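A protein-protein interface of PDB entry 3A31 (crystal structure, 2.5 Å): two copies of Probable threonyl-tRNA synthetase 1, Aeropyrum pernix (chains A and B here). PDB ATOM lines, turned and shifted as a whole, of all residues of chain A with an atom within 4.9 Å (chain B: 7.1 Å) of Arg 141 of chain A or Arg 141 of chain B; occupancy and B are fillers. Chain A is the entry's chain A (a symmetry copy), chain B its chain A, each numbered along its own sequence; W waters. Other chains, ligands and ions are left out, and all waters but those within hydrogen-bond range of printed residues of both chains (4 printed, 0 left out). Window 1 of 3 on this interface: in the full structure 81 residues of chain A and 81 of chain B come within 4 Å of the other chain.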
ATOM      1  N   ARG A  52      27.669 -20.895 -22.997  1.00  0.00           N
ATOM      2  CA  ARG A  52      26.403 -21.475 -22.505  1.00  0.00           C
ATOM      3  C   ARG A  52      25.588 -20.541 -21.635  1.00  0.00           C
ATOM      4  O   ARG A  52      24.363 -20.472 -21.790  1.00  0.00           O
ATOM      5  CB  ARG A  52      26.616 -22.809 -21.787  1.00  0.00           C
ATOM      6  CG  ARG A  52      26.824 -23.978 -22.810  1.00  0.00           C
ATOM      7  CD  ARG A  52      26.965 -25.306 -22.041  1.00  0.00           C
ATOM      8  NE  ARG A  52      25.658 -25.795 -21.564  1.00  0.00           N
ATOM      9  CZ  ARG A  52      24.751 -26.403 -22.358  1.00  0.00           C
ATOM     10  NH1 ARG A  52      24.999 -26.615 -23.665  1.00  0.00           N
ATOM     11  NH2 ARG A  52      23.583 -26.792 -21.857  1.00  0.00           N
ATOM     12  N   GLU A  72      11.845 -22.686 -15.918  1.00  0.00           N
ATOM     13  CA  GLU A  72      12.855 -23.710 -15.780  1.00  0.00           C
ATOM     14  C   GLU A  72      12.116 -24.887 -15.113  1.00  0.00           C
ATOM     15  O   GLU A  72      11.439 -24.704 -14.091  1.00  0.00           O
ATOM     16  CB  GLU A  72      14.071 -23.162 -15.006  1.00  0.00           C
ATOM     17  CG  GLU A  72      14.857 -24.212 -14.185  1.00  0.00           C
ATOM     18  CD  GLU A  72      16.396 -23.894 -14.026  1.00  0.00           C
ATOM     19  OE1 GLU A  72      16.756 -22.703 -14.121  1.00  0.00           O
ATOM     20  OE2 GLU A  72      17.241 -24.851 -13.837  1.00  0.00           O
ATOM     21  N   ILE A  75      14.407 -31.702 -13.777  1.00  0.00           N
ATOM     22  CA  ILE A  75      15.168 -32.558 -14.617  1.00  0.00           C
ATOM     23  C   ILE A  75      14.740 -34.043 -14.509  1.00  0.00           C
ATOM     24  O   ILE A  75      14.882 -34.805 -15.469  1.00  0.00           O
ATOM     25  CB  ILE A  75      16.641 -32.307 -14.285  1.00  0.00           C
ATOM     26  CG1 ILE A  75      17.034 -30.994 -14.961  1.00  0.00           C
ATOM     27  CG2 ILE A  75      17.531 -33.487 -14.729  1.00  0.00           C
ATOM     28  CD1 ILE A  75      18.458 -30.675 -14.926  1.00  0.00           C
ATOM     29  N   LYS A 108      14.203 -36.594 -17.491  1.00  0.00           N
ATOM     30  CA  LYS A 108      13.274 -36.000 -18.438  1.00  0.00           C
ATOM     31  C   LYS A 108      13.808 -36.120 -19.865  1.00  0.00           C
ATOM     32  O   LYS A 108      14.937 -35.685 -20.159  1.00  0.00           O
ATOM     33  CB  LYS A 108      13.055 -34.535 -17.992  1.00  0.00           C
ATOM     34  CG  LYS A 108      12.615 -33.507 -18.992  1.00  0.00           C
ATOM     35  CD  LYS A 108      12.377 -32.106 -18.334  1.00  0.00           C
ATOM     36  CE  LYS A 108      13.580 -31.198 -18.392  1.00  0.00           C
ATOM     37  NZ  LYS A 108      13.332 -29.767 -17.818  1.00  0.00           N
ATOM     38  N   ASN A 111      10.295 -31.635 -22.334  1.00  0.00           N
ATOM     39  CA  ASN A 111       9.799 -30.586 -21.396  1.00  0.00           C
ATOM     40  C   ASN A 111       8.287 -30.435 -21.412  1.00  0.00           C
ATOM     41  O   ASN A 111       7.702 -29.961 -20.436  1.00  0.00           O
ATOM     42  CB  ASN A 111      10.352 -29.206 -21.777  1.00  0.00           C
ATOM     43  CG  ASN A 111      11.834 -29.129 -21.682  1.00  0.00           C
ATOM     44  OD1 ASN A 111      12.499 -28.825 -22.656  1.00  0.00           O
ATOM     45  ND2 ASN A 111      12.374 -29.421 -20.515  1.00  0.00           N
ATOM     46  N   PHE A 139      15.018 -22.910 -21.803  1.00  0.00           N
ATOM     47  CA  PHE A 139      16.348 -23.367 -22.212  1.00  0.00           C
ATOM     48  C   PHE A 139      16.488 -24.707 -21.482  1.00  0.00           C
ATOM     49  O   PHE A 139      16.913 -24.751 -20.333  1.00  0.00           O
ATOM     50  CB  PHE A 139      17.383 -22.329 -21.714  1.00  0.00           C
ATOM     51  CG  PHE A 139      18.769 -22.522 -22.248  1.00  0.00           C
ATOM     52  CD1 PHE A 139      19.078 -22.204 -23.571  1.00  0.00           C
ATOM     53  CD2 PHE A 139      19.785 -23.022 -21.416  1.00  0.00           C
ATOM     54  CE1 PHE A 139      20.376 -22.426 -24.085  1.00  0.00           C
ATOM     55  CE2 PHE A 139      21.113 -23.197 -21.901  1.00  0.00           C
ATOM     56  CZ  PHE A 139      21.413 -22.912 -23.222  1.00  0.00           C
ATOM     57  N   GLY A 140      16.027 -25.796 -22.087  1.00  0.00           N
ATOM     58  CA  GLY A 140      15.709 -27.023 -21.295  1.00  0.00           C
ATOM     59  C   GLY A 140      16.707 -28.164 -21.478  1.00  0.00           C
ATOM     60  O   GLY A 140      17.302 -28.319 -22.558  1.00  0.00           O
ATOM     61  N   ARG A 141      16.919 -28.965 -20.444  1.00  0.00           N
ATOM     62  CA  ARG A 141      18.002 -29.970 -20.515  1.00  0.00           C
ATOM     63  C   ARG A 141      17.350 -31.344 -20.528  1.00  0.00           C
ATOM     64  O   ARG A 141      16.610 -31.672 -19.611  1.00  0.00           O
ATOM     65  CB  ARG A 141      18.958 -29.813 -19.353  1.00  0.00           C
ATOM     66  CG  ARG A 141      19.458 -28.372 -19.205  1.00  0.00           C
ATOM     67  CD  ARG A 141      20.511 -28.187 -18.104  1.00  0.00           C
ATOM     68  NE  ARG A 141      21.320 -26.978 -18.353  1.00  0.00           N
ATOM     69  CZ  ARG A 141      20.846 -25.739 -18.187  1.00  0.00           C
ATOM     70  NH1 ARG A 141      19.593 -25.570 -17.785  1.00  0.00           N
ATOM     71  NH2 ARG A 141      21.607 -24.687 -18.458  1.00  0.00           N
ATOM     72  N   VAL A 142      17.553 -32.072 -21.630  1.00  0.00           N
ATOM     73  CA  VAL A 142      16.884 -33.323 -21.910  1.00  0.00           C
ATOM     74  C   VAL A 142      17.869 -34.471 -22.135  1.00  0.00           C
ATOM     75  O   VAL A 142      18.995 -34.285 -22.617  1.00  0.00           O
ATOM     76  CB  VAL A 142      15.881 -33.173 -23.091  1.00  0.00           C
ATOM     77  CG1 VAL A 142      14.766 -32.178 -22.744  1.00  0.00           C
ATOM     78  CG2 VAL A 142      16.542 -32.739 -24.331  1.00  0.00           C
ATOM     79  N   HIS A 143      17.462 -35.666 -21.739  1.00  0.00           N
ATOM     80  CA  HIS A 143      18.274 -36.844 -21.900  1.00  0.00           C
ATOM     81  C   HIS A 143      17.505 -37.969 -22.565  1.00  0.00           C
ATOM     82  O   HIS A 143      16.351 -38.229 -22.240  1.00  0.00           O
ATOM     83  CB  HIS A 143      18.795 -37.308 -20.557  1.00  0.00           C
ATOM     84  CG  HIS A 143      19.719 -36.335 -19.929  1.00  0.00           C
ATOM     85  ND1 HIS A 143      19.271 -35.213 -19.254  1.00  0.00           N
ATOM     86  CD2 HIS A 143      21.068 -36.288 -19.902  1.00  0.00           C
ATOM     87  CE1 HIS A 143      20.311 -34.537 -18.809  1.00  0.00           C
ATOM     88  NE2 HIS A 143      21.412 -35.157 -19.206  1.00  0.00           N
ATOM     89  N   PHE A 160      21.359 -33.088 -23.953  1.00  0.00           N
ATOM     90  CA  PHE A 160      21.502 -31.910 -24.774  1.00  0.00           C
ATOM     91  C   PHE A 160      20.471 -30.851 -24.360  1.00  0.00           C
ATOM     92  O   PHE A 160      19.608 -31.119 -23.545  1.00  0.00           O
ATOM     93  CB  PHE A 160      21.397 -32.251 -26.276  1.00  0.00           C
ATOM     94  CG  PHE A 160      20.062 -32.823 -26.698  1.00  0.00           C
ATOM     95  CD1 PHE A 160      19.090 -32.007 -27.285  1.00  0.00           C
ATOM     96  CD2 PHE A 160      19.761 -34.186 -26.494  1.00  0.00           C
ATOM     97  CE1 PHE A 160      17.839 -32.531 -27.670  1.00  0.00           C
ATOM     98  CE2 PHE A 160      18.506 -34.711 -26.877  1.00  0.00           C
ATOM     99  CZ  PHE A 160      17.544 -33.897 -27.456  1.00  0.00           C
ATOM    100  N   THR A 161      20.558 -29.661 -24.954  1.00  0.00           N
ATOM    101  CA  THR A 161      19.731 -28.553 -24.591  1.00  0.00           C
ATOM    102  C   THR A 161      18.885 -28.122 -25.791  1.00  0.00           C
ATOM    103  O   THR A 161      19.384 -28.135 -26.923  1.00  0.00           O
ATOM    104  CB  THR A 161      20.664 -27.379 -24.148  1.00  0.00           C
ATOM    105  OG1 THR A 161      21.772 -27.922 -23.449  1.00  0.00           O
ATOM    106  CG2 THR A 161      19.927 -26.354 -23.258  1.00  0.00           C
ATOM    107  N   ARG B  52      14.983 -17.553 -11.469  1.00  0.00           N
ATOM    108  CA  ARG B  52      16.055 -18.537 -11.721  1.00  0.00           C
ATOM    109  C   ARG B  52      17.037 -18.124 -12.798  1.00  0.00           C
ATOM    110  O   ARG B  52      18.248 -18.307 -12.625  1.00  0.00           O
ATOM    111  CB  ARG B  52      15.504 -19.932 -12.019  1.00  0.00           C
ATOM    112  CG  ARG B  52      15.062 -20.662 -10.705  1.00  0.00           C
ATOM    113  CD  ARG B  52      14.580 -22.084 -11.051  1.00  0.00           C
ATOM    114  NE  ARG B  52      15.714 -22.989 -11.314  1.00  0.00           N
ATOM    115  CZ  ARG B  52      16.479 -23.533 -10.344  1.00  0.00           C
ATOM    116  NH1 ARG B  52      16.235 -23.284  -9.042  1.00  0.00           N
ATOM    117  NH2 ARG B  52      17.501 -24.319 -10.664  1.00  0.00           N
ATOM    118  N   TYR B  53      16.542 -17.527 -13.886  1.00  0.00           N
ATOM    119  CA  TYR B  53      17.477 -17.084 -14.922  1.00  0.00           C
ATOM    120  C   TYR B  53      18.290 -15.912 -14.355  1.00  0.00           C
ATOM    121  O   TYR B  53      19.505 -15.884 -14.525  1.00  0.00           O
ATOM    122  CB  TYR B  53      16.775 -16.748 -16.234  1.00  0.00           C
ATOM    123  CG  TYR B  53      16.275 -17.960 -16.976  1.00  0.00           C
ATOM    124  CD1 TYR B  53      15.061 -18.548 -16.628  1.00  0.00           C
ATOM    125  CD2 TYR B  53      17.013 -18.529 -18.046  1.00  0.00           C
ATOM    126  CE1 TYR B  53      14.575 -19.674 -17.287  1.00  0.00           C
ATOM    127  CE2 TYR B  53      16.549 -19.658 -18.744  1.00  0.00           C
ATOM    128  CZ  TYR B  53      15.302 -20.208 -18.368  1.00  0.00           C
ATOM    129  OH  TYR B  53      14.776 -21.304 -19.004  1.00  0.00           O
ATOM    130  N   ALA B  56      20.992 -17.080 -11.926  1.00  0.00           N
ATOM    131  CA  ALA B  56      22.124 -17.714 -12.597  1.00  0.00           C
ATOM    132  C   ALA B  56      23.056 -16.646 -13.187  1.00  0.00           C
ATOM    133  O   ALA B  56      24.297 -16.738 -13.067  1.00  0.00           O
ATOM    134  CB  ALA B  56      21.641 -18.636 -13.711  1.00  0.00           C
ATOM    135  N   GLU B  72      29.654 -25.076 -17.117  1.00  0.00           N
ATOM    136  CA  GLU B  72      28.424 -25.823 -16.983  1.00  0.00           C
ATOM    137  C   GLU B  72      28.837 -27.286 -17.245  1.00  0.00           C
ATOM    138  O   GLU B  72      29.500 -27.579 -18.250  1.00  0.00           O
ATOM    139  CB  GLU B  72      27.346 -25.255 -17.929  1.00  0.00           C
ATOM    140  CG  GLU B  72      26.303 -26.282 -18.431  1.00  0.00           C
ATOM    141  CD  GLU B  72      24.880 -25.668 -18.733  1.00  0.00           C
ATOM    142  OE1 GLU B  72      24.818 -24.452 -19.008  1.00  0.00           O
ATOM    143  OE2 GLU B  72      23.825 -26.408 -18.662  1.00  0.00           O
ATOM    144  N   THR B  73      28.535 -28.186 -16.319  1.00  0.00           N
ATOM    145  CA  THR B  73      29.024 -29.557 -16.474  1.00  0.00           C
ATOM    146  C   THR B  73      27.845 -30.455 -16.671  1.00  0.00           C
ATOM    147  O   THR B  73      26.755 -30.118 -16.228  1.00  0.00           O
ATOM    148  CB  THR B  73      29.962 -30.051 -15.314  1.00  0.00           C
ATOM    149  OG1 THR B  73      29.272 -30.036 -14.039  1.00  0.00           O
ATOM    150  CG2 THR B  73      31.287 -29.200 -15.292  1.00  0.00           C
ATOM    151  N   PRO B  74      28.061 -31.633 -17.289  1.00  0.00           N
ATOM    152  CA  PRO B  74      26.945 -32.543 -17.591  1.00  0.00           C
ATOM    153  C   PRO B  74      26.145 -32.982 -16.349  1.00  0.00           C
ATOM    154  O   PRO B  74      26.624 -32.948 -15.218  1.00  0.00           O
ATOM    155  CB  PRO B  74      27.658 -33.764 -18.165  1.00  0.00           C
ATOM    156  CG  PRO B  74      28.905 -33.222 -18.670  1.00  0.00           C
ATOM    157  CD  PRO B  74      29.349 -32.243 -17.642  1.00  0.00           C
ATOM    158  N   ILE B  75      24.939 -33.439 -16.588  1.00  0.00           N
ATOM    159  CA  ILE B  75      24.028 -33.800 -15.561  1.00  0.00           C
ATOM    160  C   ILE B  75      24.085 -35.308 -15.210  1.00  0.00           C
ATOM    161  O   ILE B  75      23.800 -35.695 -14.073  1.00  0.00           O
ATOM    162  CB  ILE B  75      22.646 -33.315 -16.006  1.00  0.00           C
ATOM    163  CG1 ILE B  75      22.602 -31.806 -15.764  1.00  0.00           C
ATOM    164  CG2 ILE B  75      21.517 -34.063 -15.266  1.00  0.00           C
ATOM    165  CD1 ILE B  75      21.295 -31.183 -15.944  1.00  0.00           C
ATOM    166  N   VAL B 107      22.821 -40.002 -12.199  1.00  0.00           N
ATOM    167  CA  VAL B 107      22.454 -38.585 -12.165  1.00  0.00           C
ATOM    168  C   VAL B 107      23.390 -37.932 -11.133  1.00  0.00           C
ATOM    169  O   VAL B 107      23.488 -38.368  -9.956  1.00  0.00           O
ATOM    170  CB  VAL B 107      20.979 -38.395 -11.788  1.00  0.00           C
ATOM    171  CG1 VAL B 107      20.567 -36.901 -11.868  1.00  0.00           C
ATOM    172  CG2 VAL B 107      20.107 -39.248 -12.735  1.00  0.00           C
ATOM    173  N   LYS B 108      24.107 -36.914 -11.589  1.00  0.00           N
ATOM    174  CA  LYS B 108      25.185 -36.306 -10.826  1.00  0.00           C
ATOM    175  C   LYS B 108      24.691 -35.867  -9.449  1.00  0.00           C
ATOM    176  O   LYS B 108      23.709 -35.109  -9.338  1.00  0.00           O
ATOM    177  CB  LYS B 108      25.730 -35.135 -11.678  1.00  0.00           C
ATOM    178  CG  LYS B 108      26.440 -33.993 -11.011  1.00  0.00           C
ATOM    179  CD  LYS B 108      26.980 -32.949 -12.045  1.00  0.00           C
ATOM    180  CE  LYS B 108      26.032 -31.804 -12.303  1.00  0.00           C
ATOM    181  NZ  LYS B 108      26.592 -30.710 -13.264  1.00  0.00           N
ATOM    182  N   PRO B 109      25.335 -36.347  -8.373  1.00  0.00           N
ATOM    183  CA  PRO B 109      24.965 -35.753  -7.080  1.00  0.00           C
ATOM    184  C   PRO B 109      25.866 -34.617  -6.666  1.00  0.00           C
ATOM    185  O   PRO B 109      25.565 -33.913  -5.701  1.00  0.00           O
ATOM    186  CB  PRO B 109      25.139 -36.924  -6.110  1.00  0.00           C
ATOM    187  CG  PRO B 109      26.316 -37.639  -6.623  1.00  0.00           C
ATOM    188  CD  PRO B 109      26.309 -37.444  -8.191  1.00  0.00           C
ATOM    189  N   MET B 110      26.977 -34.442  -7.358  1.00  0.00           N
ATOM    190  CA  MET B 110      27.912 -33.355  -7.024  1.00  0.00           C
ATOM    191  C   MET B 110      28.667 -33.023  -8.264  1.00  0.00           C
ATOM    192  O   MET B 110      28.704 -33.858  -9.187  1.00  0.00           O
ATOM    193  CB  MET B 110      28.897 -33.807  -5.953  1.00  0.00           C
ATOM    194  CG  MET B 110      29.664 -35.106  -6.274  1.00  0.00           C
ATOM    195  SD  MET B 110      30.647 -35.757  -4.642  1.00  0.00           S
ATOM    196  CE  MET B 110      29.590 -34.796  -3.224  1.00  0.00           C
ATOM    197  N   ASN B 111      29.259 -31.826  -8.290  1.00  0.00           N
ATOM    198  CA  ASN B 111      29.957 -31.251  -9.477  1.00  0.00           C
ATOM    199  C   ASN B 111      31.461 -31.468  -9.451  1.00  0.00           C
ATOM    200  O   ASN B 111      32.105 -31.457 -10.501  1.00  0.00           O
ATOM    201  CB  ASN B 111      29.763 -29.731  -9.542  1.00  0.00           C
ATOM    202  CG  ASN B 111      28.339 -29.334  -9.710  1.00  0.00           C
ATOM    203  OD1 ASN B 111      27.802 -28.606  -8.894  1.00  0.00           O
ATOM    204  ND2 ASN B 111      27.703 -29.821 -10.757  1.00  0.00           N
ATOM    205  N   GLU B 138      30.239 -22.950 -10.835  1.00  0.00           N
ATOM    206  CA  GLU B 138      29.069 -23.464 -11.593  1.00  0.00           C
ATOM    207  C   GLU B 138      27.757 -23.253 -10.841  1.00  0.00           C
ATOM    208  O   GLU B 138      27.693 -23.521  -9.655  1.00  0.00           O
ATOM    209  CB  GLU B 138      29.193 -24.955 -11.946  1.00  0.00           C
ATOM    210  CG  GLU B 138      27.977 -25.537 -12.696  1.00  0.00           C
ATOM    211  CD  GLU B 138      28.232 -26.944 -13.339  1.00  0.00           C
ATOM    212  OE1 GLU B 138      29.342 -27.502 -13.112  1.00  0.00           O
ATOM    213  OE2 GLU B 138      27.333 -27.506 -14.055  1.00  0.00           O
ATOM    214  N   PHE B 139      26.736 -22.786 -11.550  1.00  0.00           N
ATOM    215  CA  PHE B 139      25.352 -22.771 -11.073  1.00  0.00           C
ATOM    216  C   PHE B 139      24.869 -24.193 -11.378  1.00  0.00           C
ATOM    217  O   PHE B 139      24.405 -24.472 -12.477  1.00  0.00           O
ATOM    218  CB  PHE B 139      24.577 -21.711 -11.893  1.00  0.00           C
ATOM    219  CG  PHE B 139      23.205 -21.402 -11.377  1.00  0.00           C
ATOM    220  CD1 PHE B 139      23.030 -20.643 -10.219  1.00  0.00           C
ATOM    221  CD2 PHE B 139      22.069 -21.867 -12.060  1.00  0.00           C
ATOM    222  CE1 PHE B 139      21.736 -20.387  -9.711  1.00  0.00           C
ATOM    223  CE2 PHE B 139      20.756 -21.569 -11.595  1.00  0.00           C
ATOM    224  CZ  PHE B 139      20.582 -20.844 -10.429  1.00  0.00           C
ATOM    225  N   GLY B 140      25.080 -25.131 -10.462  1.00  0.00           N
ATOM    226  CA  GLY B 140      25.067 -26.577 -10.844  1.00  0.00           C
ATOM    227  C   GLY B 140      23.833 -27.340 -10.368  1.00  0.00           C
ATOM    228  O   GLY B 140      23.258 -27.022  -9.313  1.00  0.00           O
ATOM    229  N   ARG B 141      23.399 -28.337 -11.126  1.00  0.00           N
ATOM    230  CA  ARG B 141      22.111 -28.986 -10.801  1.00  0.00           C
ATOM    231  C   ARG B 141      22.416 -30.409 -10.358  1.00  0.00           C
ATOM    232  O   ARG B 141      23.022 -31.160 -11.109  1.00  0.00           O
ATOM    233  CB  ARG B 141      21.177 -28.957 -11.992  1.00  0.00           C
ATOM    234  CG  ARG B 141      21.031 -27.549 -12.577  1.00  0.00           C
ATOM    235  CD  ARG B 141      20.012 -27.451 -13.721  1.00  0.00           C
ATOM    236  NE  ARG B 141      19.524 -26.067 -13.871  1.00  0.00           N
ATOM    237  CZ  ARG B 141      20.274 -25.084 -14.378  1.00  0.00           C
ATOM    238  NH1 ARG B 141      21.515 -25.345 -14.766  1.00  0.00           N
ATOM    239  NH2 ARG B 141      19.796 -23.848 -14.459  1.00  0.00           N
ATOM    240  N   VAL B 142      22.086 -30.708  -9.098  1.00  0.00           N
ATOM    241  CA  VAL B 142      22.447 -31.942  -8.436  1.00  0.00           C
ATOM    242  C   VAL B 142      21.225 -32.703  -7.918  1.00  0.00           C
ATOM    243  O   VAL B 142      20.195 -32.120  -7.555  1.00  0.00           O
ATOM    244  CB  VAL B 142      23.499 -31.693  -7.317  1.00  0.00           C
ATOM    245  CG1 VAL B 142      24.805 -31.142  -7.901  1.00  0.00           C
ATOM    246  CG2 VAL B 142      23.007 -30.768  -6.286  1.00  0.00           C
ATOM    247  N   HIS B 143      21.321 -34.023  -7.928  1.00  0.00           N
ATOM    248  CA  HIS B 143      20.258 -34.870  -7.456  1.00  0.00           C
ATOM    249  C   HIS B 143      20.760 -35.898  -6.460  1.00  0.00           C
ATOM    250  O   HIS B 143      21.807 -36.510  -6.651  1.00  0.00           O
ATOM    251  CB  HIS B 143      19.593 -35.573  -8.620  1.00  0.00           C
ATOM    252  CG  HIS B 143      18.905 -34.639  -9.541  1.00  0.00           C
ATOM    253  ND1 HIS B 143      19.582 -33.907 -10.500  1.00  0.00           N
ATOM    254  CD2 HIS B 143      17.606 -34.282  -9.630  1.00  0.00           C
ATOM    255  CE1 HIS B 143      18.719 -33.165 -11.164  1.00  0.00           C
ATOM    256  NE2 HIS B 143      17.516 -33.359 -10.642  1.00  0.00           N
ATOM    257  N   GLY B 159      16.157 -32.771  -6.001  1.00  0.00           N
ATOM    258  CA  GLY B 159      16.944 -32.092  -7.065  1.00  0.00           C
ATOM    259  C   GLY B 159      17.042 -30.626  -6.673  1.00  0.00           C
ATOM    260  O   GLY B 159      16.052 -30.030  -6.276  1.00  0.00           O
ATOM    261  N   PHE B 160      18.235 -30.054  -6.720  1.00  0.00           N
ATOM    262  CA  PHE B 160      18.407 -28.687  -6.290  1.00  0.00           C
ATOM    263  C   PHE B 160      19.645 -28.076  -6.960  1.00  0.00           C
ATOM    264  O   PHE B 160      20.389 -28.771  -7.627  1.00  0.00           O
ATOM    265  CB  PHE B 160      18.483 -28.583  -4.751  1.00  0.00           C
ATOM    266  CG  PHE B 160      19.657 -29.306  -4.130  1.00  0.00           C
ATOM    267  CD1 PHE B 160      20.817 -28.609  -3.775  1.00  0.00           C
ATOM    268  CD2 PHE B 160      19.617 -30.699  -3.911  1.00  0.00           C
ATOM    269  CE1 PHE B 160      21.920 -29.278  -3.208  1.00  0.00           C
ATOM    270  CE2 PHE B 160      20.724 -31.371  -3.344  1.00  0.00           C
ATOM    271  CZ  PHE B 160      21.873 -30.676  -2.997  1.00  0.00           C
ATOM    272  N   THR B 161      19.866 -26.779  -6.748  1.00  0.00           N
ATOM    273  CA  THR B 161      20.919 -26.058  -7.392  1.00  0.00           C
ATOM    274  C   THR B 161      21.887 -25.507  -6.343  1.00  0.00           C
ATOM    275  O   THR B 161      21.442 -25.064  -5.277  1.00  0.00           O
ATOM    276  CB  THR B 161      20.278 -24.880  -8.196  1.00  0.00           C
ATOM    277  OG1 THR B 161      19.047 -25.326  -8.743  1.00  0.00           O
ATOM    278  CG2 THR B 161      21.205 -24.371  -9.322  1.00  0.00           C
ATOM    279  N   GLN B 162      23.185 -25.484  -6.663  1.00  0.00           N
ATOM    280  CA  GLN B 162      24.191 -24.863  -5.793  1.00  0.00           C
ATOM    281  C   GLN B 162      24.994 -23.796  -6.543  1.00  0.00           C
ATOM    282  O   GLN B 162      25.207 -23.914  -7.750  1.00  0.00           O
ATOM    283  CB  GLN B 162      25.211 -25.897  -5.324  1.00  0.00           C
ATOM    284  CG  GLN B 162      24.663 -27.157  -4.777  1.00  0.00           C
ATOM    285  CD  GLN B 162      25.701 -28.273  -4.800  1.00  0.00           C
ATOM    286  OE1 GLN B 162      26.278 -28.603  -5.854  1.00  0.00           O
ATOM    287  NE2 GLN B 162      25.961 -28.852  -3.641  1.00  0.00           N
HETATM  288  O   HOH W   1      23.916 -33.931 -19.114  1.00  0.00           O
HETATM  289  O   HOH W   2      15.375 -31.655 -11.183  1.00  0.00           O
HETATM  290  O   HOH W   3      23.221 -21.837 -18.732  1.00  0.00           O
HETATM  291  O   HOH W   4      18.919 -20.746 -15.099  1.00  0.00           O
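The side-chain carboxylate (OE2) of Glu 72 of chain A is in salt-bridge range of the guanidinium group (NE) of Arg 141 of chain B (2.6 Å).
The guanidinium group of Arg 52 of chain A lies within salt-bridge range of the side-chain carboxylate of Glu 72 of chain B, at 3.0 Å.
OH of Tyr 53 of chain B sits at hydrogen-bond distance from N of Phe 139 of chain A (3.2 Å).
The guanidinium group of Arg 141 of chain A is in salt-bridge range of the side-chain carboxylate of Glu 72 of chain B (2.6 Å).
The guanidinium group (NE) of Arg 52 of chain B lies within salt-bridge range of the side-chain carboxylate (OE1) of Glu 72 of chain A (3.0 Å).
The backbone NH (N) of His 143 of chain B is in hydrogen-bond range of the backbone carbonyl oxygen (O) of Lys 108 of chain B (3.0 Å).
The guanidinium group (NH2) of Arg 52 of chain B is in hydrogen-bond range of the side-chain hydroxyl (OG1) of Thr 161 of chain B, 2.7 Å away.
NH2 of Arg 52 of chain A sits at hydrogen-bond distance from OG1 of Thr 161 of chain A (2.7 Å).
The backbone carbonyl oxygen (O) of Ile 75 of chain B lies within hydrogen-bond range of the backbone NH (N) of Lys 108 of chain B, at 2.8 Å.
The backbone NH of His 143 of chain A lies within hydrogen-bond range of the backbone carbonyl oxygen of Lys 108 of chain A, 3.0 Å away.
Among the printed residues, pairs that only touch across the chains: Ile 75 of chain A with Ile 75 of chain B (3.1 Å), Arg 141 of chain A with Arg 141 of chain B (3.5 Å), Ile 75 of chain A with His 143 of chain B (3.8 Å), His 143 of chain A with Ile 75 of chain B (3.8 Å), Arg 141 of chain A with Ile 75 of chain B (3.8 Å) and Ile 75 of chain A with Arg 141 of chain B (3.8 Å).
Of the printed residues of chain A, Ile 75 of chain B touches Ile 75 (3.1 Å), Arg 141 (3.8 Å) and His 143 (3.8 Å).
Of the printed residues of chain A, Arg 52 of chain B touches Glu 72 (2.9 Å).
Of the printed residues of chain A, Glu 72 of chain B touches Arg 52 (2.9 Å) and Arg 141 (2.6 Å).
Printed residues of chain A within 4 Å of His 143 of chain B: Ile 75 (3.8 Å).
Of the printed residues of chain B, Phe 139 of chain A touches Tyr 53 (3.2 Å).
Val 142 of chain B touches none of the printed residues of chain A.
The nearest residue of chain B that does not touch Arg 141 of chain A is Tyr 53 of chain B (6.5 Å).
The nearest printed residue of chain A that does not touch Arg 141 of chain B is Phe 139 of chain A (6.6 Å).
The nearest printed residue of chain B that does not touch Glu 72 of chain A is Tyr 53 of chain B (4.2 Å).
Hydrophobic or aromatic side chains of chain B within 4 Å of the printed part of chain A: Tyr 53, Ile 75 and His 143.
Hydrophobic or aromatic side chains of chain A within 4 Å of the printed part of chain B: Ile 75, Phe 139 and His 143.
Among the printed residues, Asp or Glu carboxylates within 4 Å of a Lys or Arg side-chain nitrogen of the other chain: Arg 52 of chain A with Glu 72 of chain B, Glu 72 of chain A with Arg 52 of chain B, Glu 72 of chain A with Arg 141 of chain B and Arg 141 of chain A with Glu 72 of chain B.
Arg 52 of chain A touches Glu 72 of chain B, and with the chains exchanged Glu 72 of chain A touches Arg 52 of chain B.
Glu 72 of chain A touches Arg 141 of chain B, and with the chains exchanged Arg 141 of chain A touches Glu 72 of chain B.
Ile 75 of chain A touches Arg 141 of chain B, and with the chains exchanged Arg 141 of chain A touches Ile 75 of chain B.
Ile 75 of chain A touches His 143 of chain B, and with the chains exchanged His 143 of chain A touches Ile 75 of chain B.
Positions printed for both chains: 52, 72, 75, 108, 111, 139, 140, 141, 142, 143, 160 and 161.
Of the 11 pairs that touch across the chains among the printed residues, 10 have their exchanged pair printed and touching as well.
Water W2 lies within hydrogen-bond range of the backbone NH (N) of Ile 75 of chain A and a ring nitrogen (NE2) of His 143 of chain B.
Water W1 bridges the backbone NH (N) of Ile 75 of chain B (2.8 Å) and a ring nitrogen (NE2) of His 143 of chain A (2.8 Å).
Water W4 lies within hydrogen-bond range of OE1 of Glu 72 of chain A (3.1 Å) and NH2 of Arg 141 of chain B (3.3 Å).
Water W3 lies within hydrogen-bond range of the side-chain carboxylate (OE1) of Glu 72 of chain B (3.1 Å) and the guanidinium group (NH2) of Arg 141 of chain A (3.3 Å).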
